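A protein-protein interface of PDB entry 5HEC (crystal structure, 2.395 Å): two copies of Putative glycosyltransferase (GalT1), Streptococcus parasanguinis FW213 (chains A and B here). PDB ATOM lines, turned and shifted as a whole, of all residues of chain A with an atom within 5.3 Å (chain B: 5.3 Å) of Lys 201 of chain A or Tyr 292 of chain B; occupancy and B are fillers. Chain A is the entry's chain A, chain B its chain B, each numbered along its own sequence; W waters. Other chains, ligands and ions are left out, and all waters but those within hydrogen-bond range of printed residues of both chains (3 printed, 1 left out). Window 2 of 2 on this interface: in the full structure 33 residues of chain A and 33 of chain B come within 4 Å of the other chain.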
ATOM      1  N   ASP A 115       4.499  15.897  -9.182  1.00  0.00           N
ATOM      2  CA  ASP A 115       5.224  17.103  -8.792  1.00  0.00           C
ATOM      3  C   ASP A 115       4.279  18.125  -8.142  1.00  0.00           C
ATOM      4  O   ASP A 115       4.702  19.017  -7.414  1.00  0.00           O
ATOM      5  CB  ASP A 115       5.910  17.703 -10.009  1.00  0.00           C
ATOM      6  CG  ASP A 115       6.933  16.758 -10.622  1.00  0.00           C
ATOM      7  OD1 ASP A 115       6.931  16.577 -11.856  1.00  0.00           O
ATOM      8  OD2 ASP A 115       7.755  16.198  -9.865  1.00  0.00           O
ATOM      9  N   GLU A 176      10.916  23.236  -5.701  1.00  0.00           N
ATOM     10  CA  GLU A 176      11.867  23.447  -6.793  1.00  0.00           C
ATOM     11  C   GLU A 176      11.189  24.019  -8.047  1.00  0.00           C
ATOM     12  O   GLU A 176      11.839  24.654  -8.867  1.00  0.00           O
ATOM     13  CB  GLU A 176      12.581  22.131  -7.139  1.00  0.00           C
ATOM     14  CG  GLU A 176      11.721  21.173  -7.984  1.00  0.00           C
ATOM     15  CD  GLU A 176      12.168  19.711  -7.911  1.00  0.00           C
ATOM     16  OE1 GLU A 176      12.077  19.107  -6.811  1.00  0.00           O
ATOM     17  OE2 GLU A 176      12.592  19.167  -8.962  1.00  0.00           O
ATOM     18  N   LEU A 177       9.885  23.797  -8.195  1.00  0.00           N
ATOM     19  CA  LEU A 177       9.138  24.365  -9.327  1.00  0.00           C
ATOM     20  C   LEU A 177       9.211  25.902  -9.390  1.00  0.00           C
ATOM     21  O   LEU A 177       9.102  26.496 -10.466  1.00  0.00           O
ATOM     22  CB  LEU A 177       7.671  23.939  -9.259  1.00  0.00           C
ATOM     23  CG  LEU A 177       7.409  22.439  -9.187  1.00  0.00           C
ATOM     24  CD1 LEU A 177       5.925  22.169  -9.208  1.00  0.00           C
ATOM     25  CD2 LEU A 177       8.117  21.711 -10.325  1.00  0.00           C
ATOM     26  N   PHE A 178       9.392  26.543  -8.242  1.00  0.00           N
ATOM     27  CA  PHE A 178       9.344  28.000  -8.185  1.00  0.00           C
ATOM     28  C   PHE A 178      10.598  28.731  -8.677  1.00  0.00           C
ATOM     29  O   PHE A 178      10.649  29.964  -8.625  1.00  0.00           O
ATOM     30  CB  PHE A 178       9.014  28.446  -6.760  1.00  0.00           C
ATOM     31  CG  PHE A 178       7.565  28.308  -6.433  1.00  0.00           C
ATOM     32  CD1 PHE A 178       6.672  29.317  -6.757  1.00  0.00           C
ATOM     33  CD2 PHE A 178       7.081  27.150  -5.858  1.00  0.00           C
ATOM     34  CE1 PHE A 178       5.324  29.189  -6.477  1.00  0.00           C
ATOM     35  CE2 PHE A 178       5.736  27.017  -5.578  1.00  0.00           C
ATOM     36  CZ  PHE A 178       4.859  28.035  -5.887  1.00  0.00           C
ATOM     37  N   GLU A 179      11.591  27.986  -9.161  1.00  0.00           N
ATOM     38  CA  GLU A 179      12.769  28.610  -9.765  1.00  0.00           C
ATOM     39  C   GLU A 179      12.352  29.522 -10.927  1.00  0.00           C
ATOM     40  O   GLU A 179      11.792  29.061 -11.932  1.00  0.00           O
ATOM     41  CB  GLU A 179      13.757  27.546 -10.239  1.00  0.00           C
ATOM     42  CG  GLU A 179      15.067  28.106 -10.793  1.00  0.00           C
ATOM     43  CD  GLU A 179      15.923  27.046 -11.490  1.00  0.00           C
ATOM     44  OE1 GLU A 179      15.379  25.987 -11.876  1.00  0.00           O
ATOM     45  OE2 GLU A 179      17.143  27.266 -11.640  1.00  0.00           O
ATOM     46  N   GLY A 180      12.577  30.827 -10.759  1.00  0.00           N
ATOM     47  CA  GLY A 180      12.287  31.791 -11.804  1.00  0.00           C
ATOM     48  C   GLY A 180      10.830  32.206 -11.919  1.00  0.00           C
ATOM     49  O   GLY A 180      10.477  33.008 -12.805  1.00  0.00           O
ATOM     50  N   ILE A 181       9.980  31.678 -11.037  1.00  0.00           N
ATOM     51  CA  ILE A 181       8.554  31.996 -11.094  1.00  0.00           C
ATOM     52  C   ILE A 181       8.101  32.868  -9.919  1.00  0.00           C
ATOM     53  O   ILE A 181       8.236  32.469  -8.760  1.00  0.00           O
ATOM     54  CB  ILE A 181       7.699  30.711 -11.142  1.00  0.00           C
ATOM     55  CG1 ILE A 181       7.891  30.016 -12.491  1.00  0.00           C
ATOM     56  CG2 ILE A 181       6.236  31.031 -10.941  1.00  0.00           C
ATOM     57  CD1 ILE A 181       7.063  28.752 -12.663  1.00  0.00           C
ATOM     58  N   ARG A 197       2.155  28.442 -15.085  1.00  0.00           N
ATOM     59  CA  ARG A 197       3.594  28.325 -15.341  1.00  0.00           C
ATOM     60  C   ARG A 197       4.228  27.261 -14.433  1.00  0.00           C
ATOM     61  O   ARG A 197       5.208  26.596 -14.814  1.00  0.00           O
ATOM     62  CB  ARG A 197       4.298  29.684 -15.168  1.00  0.00           C
ATOM     63  CG  ARG A 197       3.855  30.724 -16.220  1.00  0.00           C
ATOM     64  CD  ARG A 197       4.616  32.053 -16.098  1.00  0.00           C
ATOM     65  NE  ARG A 197       4.036  32.956 -15.106  1.00  0.00           N
ATOM     66  CZ  ARG A 197       4.730  33.624 -14.176  1.00  0.00           C
ATOM     67  NH1 ARG A 197       6.056  33.481 -14.083  1.00  0.00           N
ATOM     68  NH2 ARG A 197       4.100  34.441 -13.331  1.00  0.00           N
ATOM     69  N   LEU A 198       3.675  27.106 -13.233  1.00  0.00           N
ATOM     70  CA  LEU A 198       4.068  26.026 -12.337  1.00  0.00           C
ATOM     71  C   LEU A 198       3.676  24.653 -12.913  1.00  0.00           C
ATOM     72  O   LEU A 198       4.452  23.705 -12.830  1.00  0.00           O
ATOM     73  CB  LEU A 198       3.446  26.225 -10.959  1.00  0.00           C
ATOM     74  CG  LEU A 198       3.990  27.404 -10.139  1.00  0.00           C
ATOM     75  CD1 LEU A 198       3.022  27.749  -9.009  1.00  0.00           C
ATOM     76  CD2 LEU A 198       5.415  27.128  -9.584  1.00  0.00           C
ATOM     77  N   TYR A 199       2.490  24.544 -13.508  1.00  0.00           N
ATOM     78  CA  TYR A 199       2.099  23.292 -14.169  1.00  0.00           C
ATOM     79  C   TYR A 199       3.097  22.881 -15.258  1.00  0.00           C
ATOM     80  O   TYR A 199       3.460  21.699 -15.372  1.00  0.00           O
ATOM     81  CB  TYR A 199       0.712  23.396 -14.799  1.00  0.00           C
ATOM     82  CG  TYR A 199      -0.413  23.667 -13.841  1.00  0.00           C
ATOM     83  CD1 TYR A 199      -0.389  23.153 -12.553  1.00  0.00           C
ATOM     84  CD2 TYR A 199      -1.499  24.451 -14.221  1.00  0.00           C
ATOM     85  CE1 TYR A 199      -1.410  23.402 -11.670  1.00  0.00           C
ATOM     86  CE2 TYR A 199      -2.535  24.701 -13.346  1.00  0.00           C
ATOM     87  CZ  TYR A 199      -2.476  24.180 -12.071  1.00  0.00           C
ATOM     88  OH  TYR A 199      -3.489  24.409 -11.189  1.00  0.00           O
ATOM     89  N   LEU A 200       3.535  23.856 -16.053  1.00  0.00           N
ATOM     90  CA  LEU A 200       4.419  23.577 -17.184  1.00  0.00           C
ATOM     91  C   LEU A 200       5.797  23.073 -16.734  1.00  0.00           C
ATOM     92  O   LEU A 200       6.521  22.456 -17.511  1.00  0.00           O
ATOM     93  CB  LEU A 200       4.550  24.817 -18.067  1.00  0.00           C
ATOM     94  CG  LEU A 200       3.244  25.293 -18.721  1.00  0.00           C
ATOM     95  CD1 LEU A 200       3.397  26.674 -19.375  1.00  0.00           C
ATOM     96  CD2 LEU A 200       2.701  24.272 -19.725  1.00  0.00           C
ATOM     97  N   LYS A 201       6.148  23.322 -15.478  1.00  0.00           N
ATOM     98  CA  LYS A 201       7.360  22.760 -14.882  1.00  0.00           C
ATOM     99  C   LYS A 201       7.198  21.275 -14.489  1.00  0.00           C
ATOM    100  O   LYS A 201       8.185  20.541 -14.412  1.00  0.00           O
ATOM    101  CB  LYS A 201       7.767  23.566 -13.644  1.00  0.00           C
ATOM    102  CG  LYS A 201       8.218  25.002 -13.914  1.00  0.00           C
ATOM    103  CD  LYS A 201       9.623  25.040 -14.461  1.00  0.00           C
ATOM    104  CE  LYS A 201      10.259  26.405 -14.276  1.00  0.00           C
ATOM    105  NZ  LYS A 201      10.672  26.672 -12.874  1.00  0.00           N
ATOM    106  N   ALA A 202       5.965  20.837 -14.235  1.00  0.00           N
ATOM    107  CA  ALA A 202       5.726  19.481 -13.733  1.00  0.00           C
ATOM    108  C   ALA A 202       5.805  18.396 -14.814  1.00  0.00           C
ATOM    109  O   ALA A 202       5.663  18.679 -16.002  1.00  0.00           O
ATOM    110  CB  ALA A 202       4.362  19.415 -13.042  1.00  0.00           C
ATOM    111  N   SER A 203       6.018  17.154 -14.382  1.00  0.00           N
ATOM    112  CA  SER A 203       5.939  15.978 -15.259  1.00  0.00           C
ATOM    113  C   SER A 203       4.571  15.313 -15.139  1.00  0.00           C
ATOM    114  O   SER A 203       4.026  14.812 -16.115  1.00  0.00           O
ATOM    115  CB  SER A 203       7.032  14.951 -14.917  1.00  0.00           C
ATOM    116  OG  SER A 203       8.331  15.518 -14.970  1.00  0.00           O
ATOM    117  N   MET A 248       5.492  25.997 -27.006  1.00  0.00           N
ATOM    118  CA  MET A 248       5.932  24.766 -26.377  1.00  0.00           C
ATOM    119  C   MET A 248       5.225  23.566 -27.000  1.00  0.00           C
ATOM    120  O   MET A 248       5.464  22.433 -26.614  1.00  0.00           O
ATOM    121  CB  MET A 248       5.672  24.826 -24.871  1.00  0.00           C
ATOM    122  CG  MET A 248       6.522  25.849 -24.152  1.00  0.00           C
ATOM    123  SD  MET A 248       5.874  26.235 -22.515  1.00  0.00           S
ATOM    124  CE  MET A 248       6.229  24.739 -21.597  1.00  0.00           C
ATOM    125  N   TYR A 250       1.809  22.764 -27.041  1.00  0.00           N
ATOM    126  CA  TYR A 250       0.545  22.273 -26.465  1.00  0.00           C
ATOM    127  C   TYR A 250      -0.671  22.676 -27.306  1.00  0.00           C
ATOM    128  O   TYR A 250      -0.607  23.616 -28.109  1.00  0.00           O
ATOM    129  CB  TYR A 250       0.369  22.775 -25.022  1.00  0.00           C
ATOM    130  CG  TYR A 250       1.332  22.126 -24.026  1.00  0.00           C
ATOM    131  CD1 TYR A 250       2.547  22.718 -23.701  1.00  0.00           C
ATOM    132  CD2 TYR A 250       1.021  20.911 -23.425  1.00  0.00           C
ATOM    133  CE1 TYR A 250       3.422  22.117 -22.798  1.00  0.00           C
ATOM    134  CE2 TYR A 250       1.875  20.309 -22.527  1.00  0.00           C
ATOM    135  CZ  TYR A 250       3.074  20.912 -22.221  1.00  0.00           C
ATOM    136  OH  TYR A 250       3.912  20.296 -21.333  1.00  0.00           O
ATOM    137  N   ASN B 284      11.944  33.428 -17.396  1.00  0.00           N
ATOM    138  CA  ASN B 284      11.066  32.324 -17.062  1.00  0.00           C
ATOM    139  C   ASN B 284      10.410  31.746 -18.319  1.00  0.00           C
ATOM    140  O   ASN B 284      10.453  30.537 -18.551  1.00  0.00           O
ATOM    141  CB  ASN B 284      10.017  32.777 -16.050  1.00  0.00           C
ATOM    142  CG  ASN B 284       8.929  31.757 -15.854  1.00  0.00           C
ATOM    143  OD1 ASN B 284       7.750  32.033 -16.102  1.00  0.00           O
ATOM    144  ND2 ASN B 284       9.316  30.556 -15.444  1.00  0.00           N
ATOM    145  N   ASP B 287      12.978  29.975 -20.334  1.00  0.00           N
ATOM    146  CA  ASP B 287      13.334  28.746 -19.633  1.00  0.00           C
ATOM    147  C   ASP B 287      12.305  27.638 -19.901  1.00  0.00           C
ATOM    148  O   ASP B 287      12.648  26.476 -20.081  1.00  0.00           O
ATOM    149  CB  ASP B 287      13.451  29.039 -18.133  1.00  0.00           C
ATOM    150  CG  ASP B 287      13.812  27.809 -17.309  1.00  0.00           C
ATOM    151  OD1 ASP B 287      14.546  26.930 -17.806  1.00  0.00           O
ATOM    152  OD2 ASP B 287      13.350  27.723 -16.150  1.00  0.00           O
ATOM    153  N   LEU B 288      11.035  28.008 -19.939  1.00  0.00           N
ATOM    154  CA  LEU B 288       9.975  27.036 -20.156  1.00  0.00           C
ATOM    155  C   LEU B 288      10.015  26.489 -21.572  1.00  0.00           C
ATOM    156  O   LEU B 288       9.915  25.282 -21.793  1.00  0.00           O
ATOM    157  CB  LEU B 288       8.605  27.663 -19.880  1.00  0.00           C
ATOM    158  CG  LEU B 288       8.324  27.939 -18.409  1.00  0.00           C
ATOM    159  CD1 LEU B 288       6.992  28.658 -18.254  1.00  0.00           C
ATOM    160  CD2 LEU B 288       8.347  26.636 -17.613  1.00  0.00           C
ATOM    161  N   ILE B 289      10.138  27.394 -22.529  1.00  0.00           N
ATOM    162  CA  ILE B 289      10.121  27.024 -23.933  1.00  0.00           C
ATOM    163  C   ILE B 289      11.268  26.076 -24.294  1.00  0.00           C
ATOM    164  O   ILE B 289      11.064  25.081 -24.989  1.00  0.00           O
ATOM    165  CB  ILE B 289      10.177  28.276 -24.816  1.00  0.00           C
ATOM    166  CG1 ILE B 289       8.879  29.064 -24.640  1.00  0.00           C
ATOM    167  CG2 ILE B 289      10.391  27.903 -26.275  1.00  0.00           C
ATOM    168  CD1 ILE B 289       8.837  30.352 -25.403  1.00  0.00           C
ATOM    169  N   GLU B 290      12.461  26.358 -23.783  1.00  0.00           N
ATOM    170  CA  GLU B 290      13.637  25.577 -24.137  1.00  0.00           C
ATOM    171  C   GLU B 290      13.885  24.342 -23.273  1.00  0.00           C
ATOM    172  O   GLU B 290      14.506  23.388 -23.724  1.00  0.00           O
ATOM    173  CB  GLU B 290      14.871  26.473 -24.100  1.00  0.00           C
ATOM    174  CG  GLU B 290      14.968  27.356 -25.316  1.00  0.00           C
ATOM    175  CD  GLU B 290      16.027  28.428 -25.170  1.00  0.00           C
ATOM    176  OE1 GLU B 290      16.639  28.521 -24.077  1.00  0.00           O
ATOM    177  OE2 GLU B 290      16.244  29.178 -26.152  1.00  0.00           O
ATOM    178  N   ASN B 291      13.416  24.351 -22.035  1.00  0.00           N
ATOM    179  CA  ASN B 291      13.760  23.263 -21.129  1.00  0.00           C
ATOM    180  C   ASN B 291      12.572  22.462 -20.659  1.00  0.00           C
ATOM    181  O   ASN B 291      12.731  21.458 -19.978  1.00  0.00           O
ATOM    182  CB  ASN B 291      14.514  23.806 -19.920  1.00  0.00           C
ATOM    183  CG  ASN B 291      15.824  24.442 -20.307  1.00  0.00           C
ATOM    184  OD1 ASN B 291      16.604  23.858 -21.060  1.00  0.00           O
ATOM    185  ND2 ASN B 291      16.071  25.653 -19.813  1.00  0.00           N
ATOM    186  N   TYR B 292      11.372  22.908 -21.001  1.00  0.00           N
ATOM    187  CA  TYR B 292      10.189  22.155 -20.609  1.00  0.00           C
ATOM    188  C   TYR B 292       9.181  22.021 -21.732  1.00  0.00           C
ATOM    189  O   TYR B 292       7.986  22.196 -21.494  1.00  0.00           O
ATOM    190  CB  TYR B 292       9.523  22.807 -19.395  1.00  0.00           C
ATOM    191  CG  TYR B 292      10.444  22.951 -18.201  1.00  0.00           C
ATOM    192  CD1 TYR B 292      11.300  24.043 -18.087  1.00  0.00           C
ATOM    193  CD2 TYR B 292      10.468  21.990 -17.193  1.00  0.00           C
ATOM    194  CE1 TYR B 292      12.152  24.169 -17.004  1.00  0.00           C
ATOM    195  CE2 TYR B 292      11.310  22.112 -16.103  1.00  0.00           C
ATOM    196  CZ  TYR B 292      12.153  23.199 -16.018  1.00  0.00           C
ATOM    197  OH  TYR B 292      12.990  23.339 -14.931  1.00  0.00           O
ATOM    198  N   PRO B 293       9.644  21.685 -22.957  1.00  0.00           N
ATOM    199  CA  PRO B 293       8.630  21.534 -24.004  1.00  0.00           C
ATOM    200  C   PRO B 293       7.798  20.284 -23.752  1.00  0.00           C
ATOM    201  O   PRO B 293       8.213  19.416 -22.977  1.00  0.00           O
ATOM    202  CB  PRO B 293       9.460  21.392 -25.278  1.00  0.00           C
ATOM    203  CG  PRO B 293      10.685  20.680 -24.818  1.00  0.00           C
ATOM    204  CD  PRO B 293      10.955  21.172 -23.402  1.00  0.00           C
ATOM    205  N   LYS B 294       6.645  20.213 -24.405  1.00  0.00           N
ATOM    206  CA  LYS B 294       5.694  19.130 -24.206  1.00  0.00           C
ATOM    207  C   LYS B 294       6.339  17.755 -24.370  1.00  0.00           C
ATOM    208  O   LYS B 294       7.178  17.561 -25.251  1.00  0.00           O
ATOM    209  CB  LYS B 294       4.522  19.279 -25.182  1.00  0.00           C
ATOM    210  CG  LYS B 294       3.481  18.187 -25.045  1.00  0.00           C
ATOM    211  CD  LYS B 294       2.387  18.288 -26.096  1.00  0.00           C
ATOM    212  CE  LYS B 294       1.659  16.958 -26.223  1.00  0.00           C
ATOM    213  NZ  LYS B 294       0.478  17.059 -27.113  1.00  0.00           N
HETATM  214  O   HOH W   1       5.875  21.633 -20.092  1.00  0.00           O
HETATM  215  O   HOH W   2      11.766  29.397 -14.821  1.00  0.00           O
HETATM  216  O   HOH W   3      13.569  26.080 -13.922  1.00  0.00           O
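NH1 of Arg 197 of chain A lies within hydrogen-bond range of OD1 of Asn 284 of chain B, at 3.0 Å.
The backbone NH (N) of Lys 294 of chain B is in hydrogen-bond range of the backbone carbonyl oxygen (O) of Met 248 of chain A, 3.3 Å away.
NZ of Lys 201 of chain A is in hydrogen-bond range of O of Leu 177 of chain A (2.9 Å).
The side-chain amide nitrogen (ND2) of Asn 291 of chain B lies within hydrogen-bond range of the side-chain carboxylate (OD1) of Asp 287 of chain B (2.8 Å).
The side-chain amino group of Lys 201 of chain A sits at hydrogen-bond distance from the backbone carbonyl oxygen of Glu 179 of chain A (2.8 Å).
Among the printed residues, merely in contact across the chains: Gly 180 of chain A with Asn 284 of chain B (3.3 Å), Ile 181 of chain A with Asn 284 of chain B (3.3 Å), Leu 200 of chain A with Tyr 292 of chain B (3.6 Å), Lys 201 of chain A with Asp 287 of chain B (3.8 Å), Lys 201 of chain A with Leu 288 of chain B (3.8 Å), Lys 201 of chain A with Tyr 292 of chain B (3.5 Å), Met 248 of chain A with Leu 288 of chain B (3.7 Å), Met 248 of chain A with Ile 289 of chain B (3.8 Å), Met 248 of chain A with Tyr 292 of chain B (3.1 Å) and Tyr 250 of chain A with Lys 294 of chain B (3.6 Å).
Printed residues of chain B within 4 Å of Gly 180 of chain A: Asn 284.
Of the printed residues of chain B, Leu 200 of chain A touches Tyr 292.
Lys 201 of chain A touches just these residues of chain B: Asp 287 (3.8 Å), Leu 288 (3.8 Å) and Tyr 292 (3.5 Å).
Of the printed residues of chain B, Tyr 250 of chain A touches Lys 294.
Printed residues of chain A within 4 Å of Leu 288 of chain B: Lys 201 (3.8 Å) and Met 248 (3.7 Å).
Of chain A, only Leu 200, Lys 201 and Met 248 come within 4 Å of Tyr 292 of chain B.
The nearest residue of chain B that does not touch Lys 201 of chain A is Asn 284 of chain B (4.4 Å).
The nearest residue of chain A that does not touch Tyr 292 of chain B is Tyr 250 of chain A (4.5 Å).
The nearest printed residue of chain B that does not touch Leu 200 of chain A is Leu 288 of chain B (4.2 Å).
Printed residues of chain A that touch a printed residue of chain B: Gly 180, Ile 181, Arg 197, Leu 200, Lys 201, Met 248 and Tyr 250.
Hydrophobic or aromatic side chains of chain B that line the printed part of chain A: Leu 288 and Tyr 292.
Along chain B the printed residues that touch a printed residue of chain A span positions 284 to 294.
No position is printed for both chains.
Of the 12 pairs that touch across the chains among the printed residues, none has its exchanged pair printed and touching as well.
Water W1 lies within hydrogen-bond range of O of Tyr 292 of chain B (2.6 Å), OH of Tyr 250 of chain A (2.7 Å) and O of Leu 200 of chain A (2.8 Å).
Water W2 lies within hydrogen-bond range of the side-chain carboxylate of Asp 287 of chain B, the side-chain amide nitrogen of Asn 284 of chain B and the backbone carbonyl oxygen of Glu 179 of chain A.
Water W3 lies within hydrogen-bond range of the side-chain carboxylate (OE1) of Glu 179 of chain A (2.7 Å), the side-chain carboxylate (OD2) of Asp 287 of chain B (2.8 Å), the side-chain hydroxyl (OH) of Tyr 292 of chain B (3.0 Å) and the side-chain amino group (NZ) of Lys 201 of chain A (3.1 Å).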
